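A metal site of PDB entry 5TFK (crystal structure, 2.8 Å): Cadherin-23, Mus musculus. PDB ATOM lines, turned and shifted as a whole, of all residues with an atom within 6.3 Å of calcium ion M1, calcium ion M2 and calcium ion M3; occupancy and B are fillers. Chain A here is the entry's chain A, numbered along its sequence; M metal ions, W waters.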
ATOM      1  N   GLU A  23      16.961  14.892 -26.950  1.00  0.00           N
ATOM      2  CA  GLU A  23      16.374  13.535 -27.006  1.00  0.00           C
ATOM      3  C   GLU A  23      16.088  12.884 -25.636  1.00  0.00           C
ATOM      4  O   GLU A  23      16.714  13.226 -24.627  1.00  0.00           O
ATOM      5  CB  GLU A  23      17.240  12.566 -27.859  1.00  0.00           C
ATOM      6  CG  GLU A  23      18.593  12.183 -27.241  1.00  0.00           C
ATOM      7  CD  GLU A  23      19.272  10.955 -27.871  1.00  0.00           C
ATOM      8  OE1 GLU A  23      20.475  10.726 -27.591  1.00  0.00           O
ATOM      9  OE2 GLU A  23      18.615  10.213 -28.635  1.00  0.00           O
ATOM     10  N   ASN A  24      15.131  11.941 -25.609  1.00  0.00           N
ATOM     11  CA  ASN A  24      14.660  11.328 -24.351  1.00  0.00           C
ATOM     12  C   ASN A  24      14.126  12.357 -23.359  1.00  0.00           C
ATOM     13  O   ASN A  24      14.193  12.138 -22.144  1.00  0.00           O
ATOM     14  CB  ASN A  24      15.763  10.510 -23.641  1.00  0.00           C
ATOM     15  CG  ASN A  24      16.423   9.487 -24.542  1.00  0.00           C
ATOM     16  OD1 ASN A  24      15.734   8.682 -25.181  1.00  0.00           O
ATOM     17  ND2 ASN A  24      17.747   9.516 -24.596  1.00  0.00           N
ATOM     18  N   ILE A  80      11.536  10.123 -28.087  1.00  0.00           N
ATOM     19  CA  ILE A  80      12.326  10.678 -29.177  1.00  0.00           C
ATOM     20  C   ILE A  80      13.781  10.233 -29.060  1.00  0.00           C
ATOM     21  O   ILE A  80      14.393  10.442 -27.977  1.00  0.00           O
ATOM     22  CB  ILE A  80      12.281  12.207 -29.178  1.00  0.00           C
ATOM     23  CG1 ILE A  80      10.825  12.683 -29.251  1.00  0.00           C
ATOM     24  CG2 ILE A  80      13.103  12.765 -30.344  1.00  0.00           C
ATOM     25  CD1 ILE A  80      10.644  14.175 -29.170  1.00  0.00           C
ATOM     26  N   ASP A  81      14.291   9.637 -30.142  1.00  0.00           N
ATOM     27  CA  ASP A  81      15.592   8.967 -30.146  1.00  0.00           C
ATOM     28  C   ASP A  81      16.444   9.477 -31.288  1.00  0.00           C
ATOM     29  O   ASP A  81      16.027   9.344 -32.415  1.00  0.00           O
ATOM     30  CB  ASP A  81      15.355   7.474 -30.353  1.00  0.00           C
ATOM     31  CG  ASP A  81      16.617   6.724 -30.663  1.00  0.00           C
ATOM     32  OD1 ASP A  81      17.703   7.176 -30.238  1.00  0.00           O
ATOM     33  OD2 ASP A  81      16.525   5.661 -31.289  1.00  0.00           O
ATOM     34  N   ARG A  82      17.612  10.064 -31.000  1.00  0.00           N
ATOM     35  CA  ARG A  82      18.365  10.774 -32.022  1.00  0.00           C
ATOM     36  C   ARG A  82      19.022   9.785 -32.980  1.00  0.00           C
ATOM     37  O   ARG A  82      19.338  10.111 -34.134  1.00  0.00           O
ATOM     38  CB  ARG A  82      19.410  11.658 -31.336  1.00  0.00           C
ATOM     39  CG  ARG A  82      19.971  12.751 -32.228  1.00  0.00           C
ATOM     40  CD  ARG A  82      21.279  13.314 -31.683  1.00  0.00           C
ATOM     41  NE  ARG A  82      22.244  12.240 -31.487  1.00  0.00           N
ATOM     42  CZ  ARG A  82      22.887  11.610 -32.468  1.00  0.00           C
ATOM     43  NH1 ARG A  82      22.710  11.940 -33.751  1.00  0.00           N
ATOM     44  NH2 ARG A  82      23.734  10.631 -32.162  1.00  0.00           N
ATOM     45  N   GLU A  83      19.221   8.563 -32.492  1.00  0.00           N
ATOM     46  CA  GLU A  83      19.849   7.472 -33.230  1.00  0.00           C
ATOM     47  C   GLU A  83      18.879   6.900 -34.259  1.00  0.00           C
ATOM     48  O   GLU A  83      19.275   6.063 -35.061  1.00  0.00           O
ATOM     49  CB  GLU A  83      20.269   6.345 -32.276  1.00  0.00           C
ATOM     50  CG  GLU A  83      21.472   6.627 -31.377  1.00  0.00           C
ATOM     51  CD  GLU A  83      21.302   7.842 -30.471  1.00  0.00           C
ATOM     52  OE1 GLU A  83      20.618   7.765 -29.430  1.00  0.00           O
ATOM     53  OE2 GLU A  83      21.882   8.885 -30.823  1.00  0.00           O
ATOM     54  N   ALA A  84      17.605   7.305 -34.205  1.00  0.00           N
ATOM     55  CA  ALA A  84      16.605   6.854 -35.180  1.00  0.00           C
ATOM     56  C   ALA A  84      16.316   7.901 -36.269  1.00  0.00           C
ATOM     57  O   ALA A  84      15.475   7.663 -37.136  1.00  0.00           O
ATOM     58  CB  ALA A  84      15.330   6.470 -34.453  1.00  0.00           C
ATOM     59  N   LEU A 113      18.984  17.191 -30.088  1.00  0.00           N
ATOM     60  CA  LEU A 113      20.312  17.230 -29.549  1.00  0.00           C
ATOM     61  C   LEU A 113      20.648  15.867 -28.980  1.00  0.00           C
ATOM     62  O   LEU A 113      19.760  15.039 -28.729  1.00  0.00           O
ATOM     63  CB  LEU A 113      20.447  18.328 -28.498  1.00  0.00           C
ATOM     64  CG  LEU A 113      20.410  19.754 -29.065  1.00  0.00           C
ATOM     65  CD1 LEU A 113      19.723  20.673 -28.081  1.00  0.00           C
ATOM     66  CD2 LEU A 113      21.809  20.276 -29.423  1.00  0.00           C
ATOM     67  N   ASP A 114      21.933  15.643 -28.727  1.00  0.00           N
ATOM     68  CA  ASP A 114      22.464  14.319 -28.397  1.00  0.00           C
ATOM     69  C   ASP A 114      22.597  14.132 -26.903  1.00  0.00           C
ATOM     70  O   ASP A 114      23.175  14.967 -26.213  1.00  0.00           O
ATOM     71  CB  ASP A 114      23.824  14.105 -29.037  1.00  0.00           C
ATOM     72  CG  ASP A 114      24.295  12.656 -28.951  1.00  0.00           C
ATOM     73  OD1 ASP A 114      23.446  11.741 -29.090  1.00  0.00           O
ATOM     74  OD2 ASP A 114      25.503  12.439 -28.739  1.00  0.00           O
ATOM     75  N   ASP A 115      22.030  13.027 -26.429  1.00  0.00           N
ATOM     76  CA  ASP A 115      22.158  12.559 -25.061  1.00  0.00           C
ATOM     77  C   ASP A 115      23.067  11.323 -25.064  1.00  0.00           C
ATOM     78  O   ASP A 115      22.946  10.475 -25.940  1.00  0.00           O
ATOM     79  CB  ASP A 115      20.766  12.187 -24.540  1.00  0.00           C
ATOM     80  CG  ASP A 115      20.774  11.674 -23.117  1.00  0.00           C
ATOM     81  OD1 ASP A 115      21.665  12.053 -22.322  1.00  0.00           O
ATOM     82  OD2 ASP A 115      19.847  10.894 -22.810  1.00  0.00           O
ATOM     83  N   ASN A 116      23.961  11.226 -24.104  1.00  0.00           N
ATOM     84  CA  ASN A 116      24.914  10.148 -24.081  1.00  0.00           C
ATOM     85  C   ASN A 116      24.212   8.887 -23.600  1.00  0.00           C
ATOM     86  O   ASN A 116      24.378   8.503 -22.448  1.00  0.00           O
ATOM     87  CB  ASN A 116      26.091  10.498 -23.174  1.00  0.00           C
ATOM     88  CG  ASN A 116      27.252   9.556 -23.347  1.00  0.00           C
ATOM     89  OD1 ASN A 116      27.438   8.969 -24.411  1.00  0.00           O
ATOM     90  ND2 ASN A 116      28.048   9.388 -22.285  1.00  0.00           N
ATOM     91  N   ASP A 117      23.440   8.277 -24.495  1.00  0.00           N
ATOM     92  CA  ASP A 117      22.518   7.160 -24.141  1.00  0.00           C
ATOM     93  C   ASP A 117      22.897   5.793 -24.692  1.00  0.00           C
ATOM     94  O   ASP A 117      22.133   4.837 -24.566  1.00  0.00           O
ATOM     95  CB  ASP A 117      21.055   7.473 -24.504  1.00  0.00           C
ATOM     96  CG  ASP A 117      20.798   7.648 -26.002  1.00  0.00           C
ATOM     97  OD1 ASP A 117      21.703   8.015 -26.773  1.00  0.00           O
ATOM     98  OD2 ASP A 117      19.622   7.487 -26.406  1.00  0.00           O
ATOM     99  N   ASN A 118      24.082   5.710 -25.293  1.00  0.00           N
ATOM    100  CA  ASN A 118      24.580   4.479 -25.904  1.00  0.00           C
ATOM    101  C   ASN A 118      25.973   4.153 -25.344  1.00  0.00           C
ATOM    102  O   ASN A 118      26.853   5.016 -25.319  1.00  0.00           O
ATOM    103  CB  ASN A 118      24.676   4.636 -27.427  1.00  0.00           C
ATOM    104  CG  ASN A 118      23.337   4.467 -28.124  1.00  0.00           C
ATOM    105  OD1 ASN A 118      23.076   3.435 -28.703  1.00  0.00           O
ATOM    106  ND2 ASN A 118      22.516   5.519 -28.121  1.00  0.00           N
ATOM    107  N   TRP A 119      26.159   2.890 -24.962  1.00  0.00           N
ATOM    108  CA  TRP A 119      27.372   2.378 -24.372  1.00  0.00           C
ATOM    109  C   TRP A 119      28.364   2.009 -25.484  1.00  0.00           C
ATOM    110  O   TRP A 119      28.027   1.321 -26.470  1.00  0.00           O
ATOM    111  CB  TRP A 119      27.122   1.105 -23.567  1.00  0.00           C
ATOM    112  CG  TRP A 119      26.542   1.307 -22.218  1.00  0.00           C
ATOM    113  CD1 TRP A 119      27.203   1.285 -21.035  1.00  0.00           C
ATOM    114  CD2 TRP A 119      25.163   1.506 -21.907  1.00  0.00           C
ATOM    115  NE1 TRP A 119      26.325   1.470 -20.004  1.00  0.00           N
ATOM    116  CE2 TRP A 119      25.068   1.613 -20.516  1.00  0.00           C
ATOM    117  CE3 TRP A 119      24.008   1.611 -22.678  1.00  0.00           C
ATOM    118  CZ2 TRP A 119      23.846   1.813 -19.867  1.00  0.00           C
ATOM    119  CZ3 TRP A 119      22.791   1.798 -22.041  1.00  0.00           C
ATOM    120  CH2 TRP A 119      22.724   1.900 -20.643  1.00  0.00           C
ATOM    121  N   PRO A 120      29.615   2.421 -25.322  1.00  0.00           N
ATOM    122  CA  PRO A 120      30.700   1.773 -26.102  1.00  0.00           C
ATOM    123  C   PRO A 120      30.556   0.250 -26.010  1.00  0.00           C
ATOM    124  O   PRO A 120      30.444  -0.298 -24.906  1.00  0.00           O
ATOM    125  CB  PRO A 120      31.973   2.255 -25.398  1.00  0.00           C
ATOM    126  CG  PRO A 120      31.595   3.562 -24.797  1.00  0.00           C
ATOM    127  CD  PRO A 120      30.149   3.430 -24.378  1.00  0.00           C
ATOM    128  N   ASP A 148      30.115   3.126 -30.626  1.00  0.00           N
ATOM    129  CA  ASP A 148      29.121   3.902 -29.867  1.00  0.00           C
ATOM    130  C   ASP A 148      28.201   4.668 -30.831  1.00  0.00           C
ATOM    131  O   ASP A 148      28.702   5.408 -31.691  1.00  0.00           O
ATOM    132  CB  ASP A 148      29.911   4.872 -28.959  1.00  0.00           C
ATOM    133  CG  ASP A 148      29.046   5.568 -27.899  1.00  0.00           C
ATOM    134  OD1 ASP A 148      27.893   5.974 -28.194  1.00  0.00           O
ATOM    135  OD2 ASP A 148      29.543   5.780 -26.773  1.00  0.00           O
ATOM    136  N   GLU A 149      26.897   4.415 -30.735  1.00  0.00           N
ATOM    137  CA  GLU A 149      25.950   4.962 -31.677  1.00  0.00           C
ATOM    138  C   GLU A 149      25.756   6.450 -31.456  1.00  0.00           C
ATOM    139  O   GLU A 149      25.208   7.096 -32.315  1.00  0.00           O
ATOM    140  CB  GLU A 149      24.594   4.266 -31.623  1.00  0.00           C
ATOM    141  CG  GLU A 149      24.634   2.762 -31.845  1.00  0.00           C
ATOM    142  CD  GLU A 149      25.501   2.347 -33.020  1.00  0.00           C
ATOM    143  OE1 GLU A 149      25.000   2.337 -34.169  1.00  0.00           O
ATOM    144  OE2 GLU A 149      26.683   2.003 -32.791  1.00  0.00           O
ATOM    145  N   ASP A 150      26.219   7.000 -30.346  1.00  0.00           N
ATOM    146  CA  ASP A 150      26.159   8.444 -30.137  1.00  0.00           C
ATOM    147  C   ASP A 150      27.188   9.174 -31.006  1.00  0.00           C
ATOM    148  O   ASP A 150      27.910   8.562 -31.815  1.00  0.00           O
ATOM    149  CB  ASP A 150      26.335   8.777 -28.655  1.00  0.00           C
ATOM    150  CG  ASP A 150      25.309   8.074 -27.778  1.00  0.00           C
ATOM    151  OD1 ASP A 150      24.148   7.947 -28.227  1.00  0.00           O
ATOM    152  OD2 ASP A 150      25.668   7.654 -26.645  1.00  0.00           O
ATOM    153  N   SER A 151      27.209  10.504 -30.901  1.00  0.00           N
ATOM    154  CA  SER A 151      28.034  11.327 -31.785  1.00  0.00           C
ATOM    155  C   SER A 151      28.394  12.656 -31.150  1.00  0.00           C
ATOM    156  O   SER A 151      27.696  13.154 -30.274  1.00  0.00           O
ATOM    157  CB  SER A 151      27.351  11.547 -33.143  1.00  0.00           C
ATOM    158  OG  SER A 151      26.061  12.115 -32.978  1.00  0.00           O
ATOM    159  N   LEU A 153      31.381  14.118 -28.771  1.00  0.00           N
ATOM    160  CA  LEU A 153      32.186  13.554 -27.685  1.00  0.00           C
ATOM    161  C   LEU A 153      31.504  12.321 -27.058  1.00  0.00           C
ATOM    162  O   LEU A 153      32.180  11.474 -26.474  1.00  0.00           O
ATOM    163  CB  LEU A 153      32.451  14.613 -26.611  1.00  0.00           C
ATOM    164  CG  LEU A 153      33.231  15.871 -27.025  1.00  0.00           C
ATOM    165  CD1 LEU A 153      33.212  16.939 -25.928  1.00  0.00           C
ATOM    166  CD2 LEU A 153      34.663  15.522 -27.429  1.00  0.00           C
ATOM    167  N   ASN A 154      30.186  12.218 -27.228  1.00  0.00           N
ATOM    168  CA  ASN A 154      29.421  11.060 -26.758  1.00  0.00           C
ATOM    169  C   ASN A 154      29.731   9.759 -27.494  1.00  0.00           C
ATOM    170  O   ASN A 154      29.397   8.692 -27.007  1.00  0.00           O
ATOM    171  CB  ASN A 154      27.926  11.339 -26.901  1.00  0.00           C
ATOM    172  CG  ASN A 154      27.463  12.508 -26.053  1.00  0.00           C
ATOM    173  OD1 ASN A 154      28.186  13.009 -25.166  1.00  0.00           O
ATOM    174  ND2 ASN A 154      26.241  12.951 -26.315  1.00  0.00           N
ATOM    175  N   GLY A 155      30.297   9.866 -28.701  1.00  0.00           N
ATOM    176  CA  GLY A 155      30.674   8.694 -29.499  1.00  0.00           C
ATOM    177  C   GLY A 155      32.166   8.425 -29.657  1.00  0.00           C
ATOM    178  O   GLY A 155      32.552   7.392 -30.181  1.00  0.00           O
ATOM    179  N   LEU A 157      35.956   7.612 -28.536  1.00  0.00           N
ATOM    180  CA  LEU A 157      36.299   6.486 -27.651  1.00  0.00           C
ATOM    181  C   LEU A 157      37.780   6.456 -27.316  1.00  0.00           C
ATOM    182  O   LEU A 157      38.609   6.490 -28.212  1.00  0.00           O
ATOM    183  CB  LEU A 157      35.937   5.151 -28.314  1.00  0.00           C
ATOM    184  CG  LEU A 157      34.476   4.887 -28.670  1.00  0.00           C
ATOM    185  CD1 LEU A 157      34.272   3.433 -29.070  1.00  0.00           C
ATOM    186  CD2 LEU A 157      33.580   5.262 -27.500  1.00  0.00           C
ATOM    187  N   ASP A 201      33.620   6.376 -23.716  1.00  0.00           N
ATOM    188  CA  ASP A 201      33.290   7.663 -24.334  1.00  0.00           C
ATOM    189  C   ASP A 201      33.612   8.916 -23.504  1.00  0.00           C
ATOM    190  O   ASP A 201      33.978   8.858 -22.316  1.00  0.00           O
ATOM    191  CB  ASP A 201      31.831   7.692 -24.865  1.00  0.00           C
ATOM    192  CG  ASP A 201      30.772   7.672 -23.770  1.00  0.00           C
ATOM    193  OD1 ASP A 201      30.990   8.159 -22.637  1.00  0.00           O
ATOM    194  OD2 ASP A 201      29.654   7.195 -24.049  1.00  0.00           O
ATOM    195  N   GLY A 203      31.310  11.643 -23.117  1.00  0.00           N
ATOM    196  CA  GLY A 203      30.112  12.352 -22.656  1.00  0.00           C
ATOM    197  C   GLY A 203      30.295  12.764 -21.214  1.00  0.00           C
ATOM    198  O   GLY A 203      31.087  12.148 -20.486  1.00  0.00           O
ATOM    199  N   LEU A 207      30.212   6.943 -20.302  1.00  0.00           N
ATOM    200  CA  LEU A 207      29.843   5.521 -20.364  1.00  0.00           C
ATOM    201  C   LEU A 207      30.967   4.623 -20.930  1.00  0.00           C
ATOM    202  O   LEU A 207      31.752   5.033 -21.791  1.00  0.00           O
ATOM    203  CB  LEU A 207      28.581   5.308 -21.216  1.00  0.00           C
ATOM    204  CG  LEU A 207      27.216   5.735 -20.660  1.00  0.00           C
ATOM    205  CD1 LEU A 207      26.151   5.668 -21.740  1.00  0.00           C
ATOM    206  CD2 LEU A 207      26.804   4.871 -19.487  1.00  0.00           C
HETATM  207 CA    CA M   1      22.450   9.735 -28.138  1.00  0.00          CA
HETATM  208 CA    CA M   2      18.526   7.682 -28.153  1.00  0.00          CA
HETATM  209 CA    CA M   3      27.936   7.125 -25.624  1.00  0.00          CA
HETATM  210  O   HOH W   1      19.297   5.507 -28.365  1.00  0.00           O
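ND2 of Asn 118 lies close to OD1 of Asp 117, 3.0 Å away. The side-chain amide nitrogen (ND2) of Asn 118 lies close to the side-chain carboxylate (OE1) of Glu 83. The guanidinium group of Arg 82 lies close to the side-chain carboxylate of Asp 114 (2.7 Å). The backbone NH (N) of Glu 23 sits at hydrogen-bond distance from the backbone carbonyl oxygen (O) of Leu 113 (3.3 Å). OD2 of Asp 114 is in hydrogen-bond range of N of Ser 151 (3.4 Å). OD1 of Asp 201 lies within hydrogen-bond range of N of Leu 207 (2.7 Å). ND2 of Asn 24 sits close to OD2 of Asp 117, at 3.3 Å. The side-chain carboxylate (OE2) of Glu 23 sits close to the backbone NH (N) of Arg 82, 2.6 Å away.
Of the 26 residues printed, 6 come within 4 Å of calcium ion M3.
Calcium ion M2 is bound by OD2 of Asp 117 (2.1 Å), OD1 of Asp 81 (2.3 Å), water W1 (2.3 Å), OE1 of Glu 83 (2.5 Å) and OE2 of Glu 23 (2.6 Å). Calcium ion M2 has five donor atoms within binding distance.
Calcium ion M1 is bound by OE1 of Glu 23 (2.3 Å). The side-chain carboxylate (OD1) of Asp 117 binds calcium ion M1 (2.3 Å). O of Asp 115 is bound to calcium ion M1 (2.4 Å). Calcium ion M1 is bound by OD1 of Asp 114 (2.4 Å). OD1 of Asp 150 is bound to calcium ion M1, at 2.5 Å. Calcium ion M1 is bound by OE2 of Glu 83. Slightly farther from calcium ion M1 lies the side-chain carboxylate (OE1) of Glu 83 (3.0 Å).
Six residues have an atom within 4 Å of calcium ion M1: Glu 23, Glu 83, Asp 114, Asp 115, Asp 117 and Asp 150. The nearest printed residue that does not touch calcium ion M1 is Arg 82 (4.2 Å).
Arg 82 touches calcium ion M2 (N to CA, 3.8 Å). Within 4 Å of calcium ion M2: Glu 23, Asp 81, Arg 82, Glu 83 and Asp 117.
Calcium ion M3 is bound by the side-chain amide oxygen (OD1) of Asn 116 (2.3 Å), the side-chain carboxylate (OD2) of Asp 201 (2.3 Å), the side-chain carboxylate (OD2) of Asp 148 (2.4 Å), the backbone carbonyl oxygen (O) of Asn 118 (2.4 Å), the side-chain carboxylate (OD2) of Asp 150 (2.5 Å), the backbone carbonyl oxygen (O) of Asn 154 (2.6 Å) and the side-chain carboxylate (OD1) of Asp 148 (2.8 Å). Calcium ion M3 has seven donor atoms within binding distance.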
